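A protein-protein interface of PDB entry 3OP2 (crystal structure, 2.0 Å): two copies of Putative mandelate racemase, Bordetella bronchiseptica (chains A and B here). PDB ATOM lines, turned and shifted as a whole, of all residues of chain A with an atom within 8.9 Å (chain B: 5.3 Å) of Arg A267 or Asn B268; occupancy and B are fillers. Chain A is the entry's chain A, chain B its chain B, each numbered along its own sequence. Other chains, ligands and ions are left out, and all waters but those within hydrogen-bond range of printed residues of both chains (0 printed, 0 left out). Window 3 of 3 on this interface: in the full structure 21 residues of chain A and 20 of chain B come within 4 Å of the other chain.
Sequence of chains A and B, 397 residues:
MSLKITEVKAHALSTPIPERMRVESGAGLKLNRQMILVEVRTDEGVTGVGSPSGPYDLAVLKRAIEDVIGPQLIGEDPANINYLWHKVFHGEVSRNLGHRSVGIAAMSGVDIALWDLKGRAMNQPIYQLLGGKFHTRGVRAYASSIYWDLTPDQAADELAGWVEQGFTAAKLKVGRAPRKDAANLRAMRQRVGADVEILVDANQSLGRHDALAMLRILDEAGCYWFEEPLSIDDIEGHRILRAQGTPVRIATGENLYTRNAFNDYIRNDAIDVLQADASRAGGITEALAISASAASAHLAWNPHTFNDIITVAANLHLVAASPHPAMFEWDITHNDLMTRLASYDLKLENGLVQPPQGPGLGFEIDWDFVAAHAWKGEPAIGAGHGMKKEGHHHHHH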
ATOM      1  N   ILE A 235       4.742  25.745 -27.844  1.00  0.00           N
ATOM      2  CA  ILE A 235       5.914  25.154 -27.186  1.00  0.00           C
ATOM      3  C   ILE A 235       6.984  24.685 -28.194  1.00  0.00           C
ATOM      4  O   ILE A 235       8.182  24.910 -28.005  1.00  0.00           O
ATOM      5  CB  ILE A 235       5.472  23.991 -26.255  1.00  0.00           C
ATOM      6  CG1 ILE A 235       4.463  24.534 -25.234  1.00  0.00           C
ATOM      7  CG2 ILE A 235       6.682  23.325 -25.597  1.00  0.00           C
ATOM      8  CD1 ILE A 235       4.247  23.692 -24.020  1.00  0.00           C
ATOM      9  N   ARG A 239      11.023  25.504 -28.739  1.00  0.00           N
ATOM     10  CA  ARG A 239      12.034  24.454 -28.883  1.00  0.00           C
ATOM     11  C   ARG A 239      12.891  24.728 -30.122  1.00  0.00           C
ATOM     12  O   ARG A 239      14.113  24.679 -30.067  1.00  0.00           O
ATOM     13  CB  ARG A 239      11.377  23.076 -29.011  1.00  0.00           C
ATOM     14  CG  ARG A 239      12.416  21.923 -29.056  1.00  0.00           C
ATOM     15  CD  ARG A 239      11.838  20.558 -29.485  1.00  0.00           C
ATOM     16  NE  ARG A 239      11.411  20.528 -30.882  1.00  0.00           N
ATOM     17  CZ  ARG A 239      12.224  20.469 -31.946  1.00  0.00           C
ATOM     18  NH1 ARG A 239      13.548  20.449 -31.801  1.00  0.00           N
ATOM     19  NH2 ARG A 239      11.703  20.446 -33.170  1.00  0.00           N
ATOM     20  N   ARG A 242      15.222  27.608 -29.368  1.00  0.00           N
ATOM     21  CA  ARG A 242      16.274  27.106 -28.494  1.00  0.00           C
ATOM     22  C   ARG A 242      17.268  26.190 -29.220  1.00  0.00           C
ATOM     23  O   ARG A 242      18.478  26.239 -28.953  1.00  0.00           O
ATOM     24  CB  ARG A 242      15.668  26.402 -27.279  1.00  0.00           C
ATOM     25  CG  ARG A 242      16.637  26.223 -26.148  1.00  0.00           C
ATOM     26  CD  ARG A 242      15.917  25.754 -24.912  1.00  0.00           C
ATOM     27  NE  ARG A 242      16.809  25.151 -23.936  1.00  0.00           N
ATOM     28  CZ  ARG A 242      17.150  23.862 -23.912  1.00  0.00           C
ATOM     29  NH1 ARG A 242      16.700  23.013 -24.826  1.00  0.00           N
ATOM     30  NH2 ARG A 242      17.962  23.424 -22.962  1.00  0.00           N
ATOM     31  N   ARG A 259       2.630  24.703 -12.692  1.00  0.00           N
ATOM     32  CA  ARG A 259       3.789  23.820 -12.797  1.00  0.00           C
ATOM     33  C   ARG A 259       3.719  23.019 -14.084  1.00  0.00           C
ATOM     34  O   ARG A 259       4.742  22.754 -14.719  1.00  0.00           O
ATOM     35  CB  ARG A 259       3.832  22.824 -11.623  1.00  0.00           C
ATOM     36  CG  ARG A 259       4.891  23.104 -10.569  1.00  0.00           C
ATOM     37  CD  ARG A 259       5.465  21.796  -9.975  1.00  0.00           C
ATOM     38  NE  ARG A 259       4.746  21.361  -8.778  1.00  0.00           N
ATOM     39  CZ  ARG A 259       5.277  20.642  -7.786  1.00  0.00           C
ATOM     40  NH1 ARG A 259       6.556  20.264  -7.820  1.00  0.00           N
ATOM     41  NH2 ARG A 259       4.527  20.312  -6.740  1.00  0.00           N
ATOM     42  N   ASN A 260       2.501  22.617 -14.440  1.00  0.00           N
ATOM     43  CA  ASN A 260       2.268  21.762 -15.581  1.00  0.00           C
ATOM     44  C   ASN A 260       2.702  22.410 -16.897  1.00  0.00           C
ATOM     45  O   ASN A 260       3.319  21.755 -17.742  1.00  0.00           O
ATOM     46  CB  ASN A 260       0.795  21.377 -15.640  1.00  0.00           C
ATOM     47  CG  ASN A 260       0.516  20.348 -16.700  1.00  0.00           C
ATOM     48  OD1 ASN A 260       0.126  20.689 -17.819  1.00  0.00           O
ATOM     49  ND2 ASN A 260       0.742  19.076 -16.371  1.00  0.00           N
ATOM     50  N   ALA A 261       2.364  23.692 -17.061  1.00  0.00           N
ATOM     51  CA  ALA A 261       2.756  24.455 -18.240  1.00  0.00           C
ATOM     52  C   ALA A 261       4.275  24.567 -18.324  1.00  0.00           C
ATOM     53  O   ALA A 261       4.851  24.359 -19.388  1.00  0.00           O
ATOM     54  CB  ALA A 261       2.099  25.847 -18.238  1.00  0.00           C
ATOM     55  N   PHE A 262       4.918  24.870 -17.200  1.00  0.00           N
ATOM     56  CA  PHE A 262       6.381  24.930 -17.153  1.00  0.00           C
ATOM     57  C   PHE A 262       7.034  23.572 -17.398  1.00  0.00           C
ATOM     58  O   PHE A 262       8.031  23.488 -18.120  1.00  0.00           O
ATOM     59  CB  PHE A 262       6.873  25.587 -15.854  1.00  0.00           C
ATOM     60  CG  PHE A 262       6.642  27.069 -15.825  1.00  0.00           C
ATOM     61  CD1 PHE A 262       7.499  27.934 -16.511  1.00  0.00           C
ATOM     62  CD2 PHE A 262       5.543  27.600 -15.157  1.00  0.00           C
ATOM     63  CE1 PHE A 262       7.275  29.306 -16.511  1.00  0.00           C
ATOM     64  CE2 PHE A 262       5.316  28.971 -15.146  1.00  0.00           C
ATOM     65  CZ  PHE A 262       6.180  29.825 -15.830  1.00  0.00           C
ATOM     66  N   ASN A 263       6.458  22.516 -16.832  1.00  0.00           N
ATOM     67  CA  ASN A 263       6.927  21.143 -17.086  1.00  0.00           C
ATOM     68  C   ASN A 263       6.877  20.784 -18.566  1.00  0.00           C
ATOM     69  O   ASN A 263       7.822  20.210 -19.104  1.00  0.00           O
ATOM     70  CB  ASN A 263       6.094  20.133 -16.299  1.00  0.00           C
ATOM     71  CG  ASN A 263       6.397  20.144 -14.811  1.00  0.00           C
ATOM     72  OD1 ASN A 263       5.566  19.710 -13.998  1.00  0.00           O
ATOM     73  ND2 ASN A 263       7.580  20.641 -14.441  1.00  0.00           N
ATOM     74  N   ASP A 264       5.767  21.132 -19.214  1.00  0.00           N
ATOM     75  CA  ASP A 264       5.599  20.956 -20.657  1.00  0.00           C
ATOM     76  C   ASP A 264       6.750  21.627 -21.420  1.00  0.00           C
ATOM     77  O   ASP A 264       7.331  21.022 -22.300  1.00  0.00           O
ATOM     78  CB  ASP A 264       4.243  21.530 -21.092  1.00  0.00           C
ATOM     79  CG  ASP A 264       3.697  20.905 -22.379  1.00  0.00           C
ATOM     80  OD1 ASP A 264       4.392  20.106 -23.053  1.00  0.00           O
ATOM     81  OD2 ASP A 264       2.542  21.238 -22.728  1.00  0.00           O
ATOM     82  N   TYR A 265       7.087  22.869 -21.075  1.00  0.00           N
ATOM     83  CA  TYR A 265       8.226  23.560 -21.710  1.00  0.00           C
ATOM     84  C   TYR A 265       9.563  22.860 -21.480  1.00  0.00           C
ATOM     85  O   TYR A 265      10.356  22.708 -22.414  1.00  0.00           O
ATOM     86  CB  TYR A 265       8.326  25.022 -21.254  1.00  0.00           C
ATOM     87  CG  TYR A 265       7.506  25.977 -22.085  1.00  0.00           C
ATOM     88  CD1 TYR A 265       6.160  26.197 -21.799  1.00  0.00           C
ATOM     89  CD2 TYR A 265       8.079  26.663 -23.156  1.00  0.00           C
ATOM     90  CE1 TYR A 265       5.392  27.084 -22.572  1.00  0.00           C
ATOM     91  CE2 TYR A 265       7.332  27.544 -23.931  1.00  0.00           C
ATOM     92  CZ  TYR A 265       5.987  27.747 -23.632  1.00  0.00           C
ATOM     93  OH  TYR A 265       5.243  28.618 -24.380  1.00  0.00           O
ATOM     94  N   ILE A 266       9.806  22.450 -20.233  1.00  0.00           N
ATOM     95  CA  ILE A 266      11.029  21.731 -19.868  1.00  0.00           C
ATOM     96  C   ILE A 266      11.151  20.399 -20.612  1.00  0.00           C
ATOM     97  O   ILE A 266      12.172  20.141 -21.242  1.00  0.00           O
ATOM     98  CB  ILE A 266      11.132  21.497 -18.333  1.00  0.00           C
ATOM     99  CG1 ILE A 266      11.280  22.841 -17.601  1.00  0.00           C
ATOM    100  CG2 ILE A 266      12.311  20.554 -17.996  1.00  0.00           C
ATOM    101  CD1 ILE A 266      11.303  22.729 -16.075  1.00  0.00           C
ATOM    102  N   ARG A 267      10.100  19.579 -20.541  1.00  0.00           N
ATOM    103  CA  ARG A 267      10.038  18.254 -21.190  1.00  0.00           C
ATOM    104  C   ARG A 267      10.374  18.333 -22.673  1.00  0.00           C
ATOM    105  O   ARG A 267      10.924  17.401 -23.256  1.00  0.00           O
ATOM    106  CB  ARG A 267       8.626  17.656 -21.039  1.00  0.00           C
ATOM    107  CG  ARG A 267       8.332  16.974 -19.697  1.00  0.00           C
ATOM    108  CD  ARG A 267       6.841  17.076 -19.282  1.00  0.00           C
ATOM    109  NE  ARG A 267       5.897  16.763 -20.365  1.00  0.00           N
ATOM    110  CZ  ARG A 267       4.625  17.165 -20.404  1.00  0.00           C
ATOM    111  NH1 ARG A 267       3.856  16.822 -21.432  1.00  0.00           N
ATOM    112  NH2 ARG A 267       4.115  17.910 -19.424  1.00  0.00           N
ATOM    113  N   ASN A 268      10.013  19.457 -23.279  1.00  0.00           N
ATOM    114  CA  ASN A 268      10.173  19.648 -24.696  1.00  0.00           C
ATOM    115  C   ASN A 268      11.419  20.441 -25.068  1.00  0.00           C
ATOM    116  O   ASN A 268      11.510  20.898 -26.197  1.00  0.00           O
ATOM    117  CB  ASN A 268       8.915  20.309 -25.262  1.00  0.00           C
ATOM    118  CG  ASN A 268       7.747  19.342 -25.336  1.00  0.00           C
ATOM    119  OD1 ASN A 268       7.784  18.393 -26.112  1.00  0.00           O
ATOM    120  ND2 ASN A 268       6.714  19.563 -24.516  1.00  0.00           N
ATOM    121  N   ASP A 269      12.367  20.598 -24.135  1.00  0.00           N
ATOM    122  CA  ASP A 269      13.629  21.338 -24.404  1.00  0.00           C
ATOM    123  C   ASP A 269      13.372  22.730 -24.990  1.00  0.00           C
ATOM    124  O   ASP A 269      14.084  23.177 -25.911  1.00  0.00           O
ATOM    125  CB  ASP A 269      14.531  20.552 -25.373  1.00  0.00           C
ATOM    126  CG  ASP A 269      14.935  19.188 -24.830  1.00  0.00           C
ATOM    127  OD1 ASP A 269      15.189  19.074 -23.618  1.00  0.00           O
ATOM    128  OD2 ASP A 269      14.997  18.224 -25.622  1.00  0.00           O
ATOM    129  N   ALA A 270      12.353  23.398 -24.457  1.00  0.00           N
ATOM    130  CA  ALA A 270      11.777  24.590 -25.090  1.00  0.00           C
ATOM    131  C   ALA A 270      12.063  25.904 -24.358  1.00  0.00           C
ATOM    132  O   ALA A 270      11.667  26.975 -24.817  1.00  0.00           O
ATOM    133  CB  ALA A 270      10.272  24.398 -25.263  1.00  0.00           C
ATOM    134  N   ILE A 271      12.771  25.832 -23.239  1.00  0.00           N
ATOM    135  CA  ILE A 271      12.937  27.003 -22.384  1.00  0.00           C
ATOM    136  C   ILE A 271      14.329  27.048 -21.730  1.00  0.00           C
ATOM    137  O   ILE A 271      14.881  26.003 -21.371  1.00  0.00           O
ATOM    138  CB  ILE A 271      11.782  27.034 -21.317  1.00  0.00           C
ATOM    139  CG1 ILE A 271      11.671  28.406 -20.639  1.00  0.00           C
ATOM    140  CG2 ILE A 271      11.914  25.858 -20.316  1.00  0.00           C
ATOM    141  CD1 ILE A 271      10.360  28.595 -19.890  1.00  0.00           C
ATOM    142  N   SER A 293      12.401  23.024  -9.968  1.00  0.00           N
ATOM    143  CA  SER A 293      12.343  22.334 -11.260  1.00  0.00           C
ATOM    144  C   SER A 293      13.270  22.958 -12.299  1.00  0.00           C
ATOM    145  O   SER A 293      13.896  22.245 -13.093  1.00  0.00           O
ATOM    146  CB  SER A 293      10.908  22.272 -11.798  1.00  0.00           C
ATOM    147  OG  SER A 293      10.550  23.474 -12.471  1.00  0.00           O
ATOM    148  N   ALA A 297      16.757  20.927 -13.861  1.00  0.00           N
ATOM    149  CA  ALA A 297      17.029  20.835 -15.292  1.00  0.00           C
ATOM    150  C   ALA A 297      18.172  21.744 -15.754  1.00  0.00           C
ATOM    151  O   ALA A 297      18.368  21.919 -16.960  1.00  0.00           O
ATOM    152  CB  ALA A 297      15.748  21.132 -16.092  1.00  0.00           C
ATOM    153  N   LEU A 299      18.351  24.904 -15.703  1.00  0.00           N
ATOM    154  CA  LEU A 299      17.817  26.112 -16.323  1.00  0.00           C
ATOM    155  C   LEU A 299      17.743  27.200 -15.262  1.00  0.00           C
ATOM    156  O   LEU A 299      18.016  26.922 -14.083  1.00  0.00           O
ATOM    157  CB  LEU A 299      16.427  25.828 -16.887  1.00  0.00           C
ATOM    158  CG  LEU A 299      16.341  24.622 -17.813  1.00  0.00           C
ATOM    159  CD1 LEU A 299      14.881  24.396 -18.240  1.00  0.00           C
ATOM    160  CD2 LEU A 299      17.270  24.793 -19.025  1.00  0.00           C
ATOM    161  N   ILE B 235       0.198  13.375 -17.563  1.00  0.00           N
ATOM    162  CA  ILE B 235       0.030  12.903 -18.932  1.00  0.00           C
ATOM    163  C   ILE B 235       0.695  11.541 -19.112  1.00  0.00           C
ATOM    164  O   ILE B 235       0.136  10.634 -19.745  1.00  0.00           O
ATOM    165  CB  ILE B 235       0.641  13.921 -19.916  1.00  0.00           C
ATOM    166  CG1 ILE B 235      -0.040  15.282 -19.740  1.00  0.00           C
ATOM    167  CG2 ILE B 235       0.543  13.417 -21.351  1.00  0.00           C
ATOM    168  CD1 ILE B 235       0.560  16.401 -20.578  1.00  0.00           C
ATOM    169  N   ARG B 239      -0.450   7.776 -20.493  1.00  0.00           N
ATOM    170  CA  ARG B 239       0.274   7.056 -21.550  1.00  0.00           C
ATOM    171  C   ARG B 239       0.511   5.611 -21.120  1.00  0.00           C
ATOM    172  O   ARG B 239       0.333   4.671 -21.901  1.00  0.00           O
ATOM    173  CB  ARG B 239       1.619   7.742 -21.855  1.00  0.00           C
ATOM    174  CG  ARG B 239       2.349   7.192 -23.088  1.00  0.00           C
ATOM    175  CD  ARG B 239       3.855   7.513 -23.095  1.00  0.00           C
ATOM    176  NE  ARG B 239       4.587   6.846 -22.008  1.00  0.00           N
ATOM    177  CZ  ARG B 239       4.929   5.553 -21.987  1.00  0.00           C
ATOM    178  NH1 ARG B 239       5.601   5.056 -20.947  1.00  0.00           N
ATOM    179  NH2 ARG B 239       4.606   4.738 -22.990  1.00  0.00           N
ATOM    180  N   ASN B 263      -3.548  18.799 -27.186  1.00  0.00           N
ATOM    181  CA  ASN B 263      -2.442  18.429 -28.066  1.00  0.00           C
ATOM    182  C   ASN B 263      -1.342  17.711 -27.307  1.00  0.00           C
ATOM    183  O   ASN B 263      -0.755  16.752 -27.809  1.00  0.00           O
ATOM    184  CB  ASN B 263      -1.876  19.656 -28.781  1.00  0.00           C
ATOM    185  CG  ASN B 263      -2.727  20.090 -29.966  1.00  0.00           C
ATOM    186  OD1 ASN B 263      -3.581  19.337 -30.455  1.00  0.00           O
ATOM    187  ND2 ASN B 263      -2.491  21.310 -30.439  1.00  0.00           N
ATOM    188  N   ASP B 264      -1.085  18.169 -26.088  1.00  0.00           N
ATOM    189  CA  ASP B 264      -0.074  17.558 -25.240  1.00  0.00           C
ATOM    190  C   ASP B 264      -0.459  16.125 -24.868  1.00  0.00           C
ATOM    191  O   ASP B 264       0.403  15.253 -24.804  1.00  0.00           O
ATOM    192  CB  ASP B 264       0.189  18.433 -24.017  1.00  0.00           C
ATOM    193  CG  ASP B 264       0.260  19.918 -24.375  1.00  0.00           C
ATOM    194  OD1 ASP B 264       1.128  20.327 -25.194  1.00  0.00           O
ATOM    195  OD2 ASP B 264      -0.575  20.683 -23.854  1.00  0.00           O
ATOM    196  N   TYR B 265      -1.751  15.874 -24.661  1.00  0.00           N
ATOM    197  CA  TYR B 265      -2.239  14.495 -24.532  1.00  0.00           C
ATOM    198  C   TYR B 265      -2.054  13.682 -25.817  1.00  0.00           C
ATOM    199  O   TYR B 265      -1.561  12.552 -25.774  1.00  0.00           O
ATOM    200  CB  TYR B 265      -3.695  14.449 -24.049  1.00  0.00           C
ATOM    201  CG  TYR B 265      -3.780  14.403 -22.546  1.00  0.00           C
ATOM    202  CD1 TYR B 265      -3.770  15.580 -21.800  1.00  0.00           C
ATOM    203  CD2 TYR B 265      -3.822  13.186 -21.865  1.00  0.00           C
ATOM    204  CE1 TYR B 265      -3.823  15.551 -20.425  1.00  0.00           C
ATOM    205  CE2 TYR B 265      -3.871  13.147 -20.486  1.00  0.00           C
ATOM    206  CZ  TYR B 265      -3.873  14.339 -19.774  1.00  0.00           C
ATOM    207  OH  TYR B 265      -3.924  14.341 -18.408  1.00  0.00           O
ATOM    208  N   ILE B 266      -2.438  14.264 -26.950  1.00  0.00           N
ATOM    209  CA  ILE B 266      -2.287  13.593 -28.246  1.00  0.00           C
ATOM    210  C   ILE B 266      -0.816  13.252 -28.541  1.00  0.00           C
ATOM    211  O   ILE B 266      -0.473  12.067 -28.664  1.00  0.00           O
ATOM    212  CB  ILE B 266      -2.917  14.403 -29.415  1.00  0.00           C
ATOM    213  CG1 ILE B 266      -4.437  14.521 -29.219  1.00  0.00           C
ATOM    214  CG2 ILE B 266      -2.576  13.750 -30.759  1.00  0.00           C
ATOM    215  CD1 ILE B 266      -5.201  15.146 -30.392  1.00  0.00           C
ATOM    216  N   ARG B 267       0.039  14.279 -28.620  1.00  0.00           N
ATOM    217  CA  ARG B 267       1.469  14.115 -28.913  1.00  0.00           C
ATOM    218  C   ARG B 267       2.076  12.966 -28.121  1.00  0.00           C
ATOM    219  O   ARG B 267       2.920  12.229 -28.629  1.00  0.00           O
ATOM    220  CB  ARG B 267       2.260  15.387 -28.567  1.00  0.00           C
ATOM    221  CG  ARG B 267       1.903  16.654 -29.349  1.00  0.00           C
ATOM    222  CD  ARG B 267       2.712  17.877 -28.843  1.00  0.00           C
ATOM    223  NE  ARG B 267       2.811  17.925 -27.378  1.00  0.00           N
ATOM    224  CZ  ARG B 267       3.401  18.895 -26.674  1.00  0.00           C
ATOM    225  NH1 ARG B 267       3.428  18.813 -25.348  1.00  0.00           N
ATOM    226  NH2 ARG B 267       3.965  19.941 -27.279  1.00  0.00           N
ATOM    227  N   ASN B 268       1.645  12.826 -26.872  1.00  0.00           N
ATOM    228  CA  ASN B 268       2.227  11.845 -25.985  1.00  0.00           C
ATOM    229  C   ASN B 268       1.543  10.477 -26.026  1.00  0.00           C
ATOM    230  O   ASN B 268       1.811   9.648 -25.171  1.00  0.00           O
ATOM    231  CB  ASN B 268       2.309  12.394 -24.550  1.00  0.00           C
ATOM    232  CG  ASN B 268       3.455  13.386 -24.364  1.00  0.00           C
ATOM    233  OD1 ASN B 268       4.618  12.993 -24.275  1.00  0.00           O
ATOM    234  ND2 ASN B 268       3.129  14.673 -24.303  1.00  0.00           N
ATOM    235  N   ASP B 269       0.682  10.236 -27.020  1.00  0.00           N
ATOM    236  CA  ASP B 269      -0.048   8.950 -27.121  1.00  0.00           C
ATOM    237  C   ASP B 269      -0.743   8.623 -25.797  1.00  0.00           C
ATOM    238  O   ASP B 269      -0.665   7.485 -25.300  1.00  0.00           O
ATOM    239  CB  ASP B 269       0.920   7.802 -27.458  1.00  0.00           C
ATOM    240  CG  ASP B 269       1.462   7.877 -28.864  1.00  0.00           C
ATOM    241  OD1 ASP B 269       0.833   8.531 -29.720  1.00  0.00           O
ATOM    242  OD2 ASP B 269       2.526   7.259 -29.112  1.00  0.00           O
ATOM    243  N   ALA B 270      -1.388   9.623 -25.211  1.00  0.00           N
ATOM    244  CA  ALA B 270      -1.819   9.512 -23.818  1.00  0.00           C
ATOM    245  C   ALA B 270      -3.320   9.293 -23.622  1.00  0.00           C
ATOM    246  O   ALA B 270      -3.775   9.035 -22.502  1.00  0.00           O
ATOM    247  CB  ALA B 270      -1.362  10.744 -23.030  1.00  0.00           C
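Of the 10 printed residues of chain B, 4 touch a printed residue of chain A. Among the printed residues, 5 pairs touch across the chains. Among the printed residues, Asp or Glu carboxylates within 4 Å of a Lys or Arg side-chain nitrogen of the other chain: Asp A264 with Arg B267.
Phe A262 touches none of the printed residues of chain B. Asn A263 touches none of the printed residues of chain B. Of the printed residues of chain B, Asp A264 touches Asp B264 and Arg B267. Printed residues of chain B within 4 Å of Arg A267: Ile B235 (3.4 Å) and Asn B268 (3.7 Å). Of the printed residues of chain A, Asp B264 touches Asp A264 (3.0 Å). Printed residues of chain A within 4 Å of Asn B268: Arg A267. Asp B269 touches none of the printed residues of chain A. The nearest residue of chain B that does not touch Arg A267 is Arg B267 (4.4 Å). The nearest printed residue of chain B that does not touch Asp A264 is Ile B235 (5.7 Å).
The side-chain carboxylate (OD1) of Asp A264 is in salt-bridge range of the guanidinium group (NH1) of Arg B267, 2.8 Å away. The side-chain amide nitrogen of Asn A268 sits close to the guanidinium group of Arg B267, at 3.5 Å. The side-chain carboxylate (OD2) of Asp A264 lies close to the side-chain carboxylate (OD1) of Asp B264, 3.0 Å away.
The side-chain carboxylate (OD1) of Asp A264 is in salt-bridge range of the guanidinium group (NH1) of Arg A267. The side-chain amide nitrogen (ND2) of Asn A268 sits at hydrogen-bond distance from the backbone carbonyl oxygen (O) of Asp A264 (2.7 Å). NH1 of Arg B267 lies within salt-bridge range of OD1 of Asp B264 (2.8 Å). The backbone carbonyl oxygen (O) of Asp B264 lies within hydrogen-bond range of the side-chain amide nitrogen (ND2) of Asn B268 (2.8 Å).
Ile B235 touches Arg A267 (CD1 to NH1, 3.4 Å). NH1 of Arg A267 touches ND2 of Asn B268, 3.7 Å away.
Asp A264 touches its own counterpart, Asp B264. Asp A264 touches Arg B267, but with the chains exchanged Arg A267 does not touch Asp B264 (4.8 Å). Arg A267 touches Ile B235, but with the chains exchanged Ile A235 does not touch Arg B267 (4.4 Å). Arg A267 touches Asn B268, and with the chains exchanged Asn A268 touches Arg B267. Of the 5 pairs that touch across the chains among the printed residues, 3 have their exchanged pair printed and touching as well.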
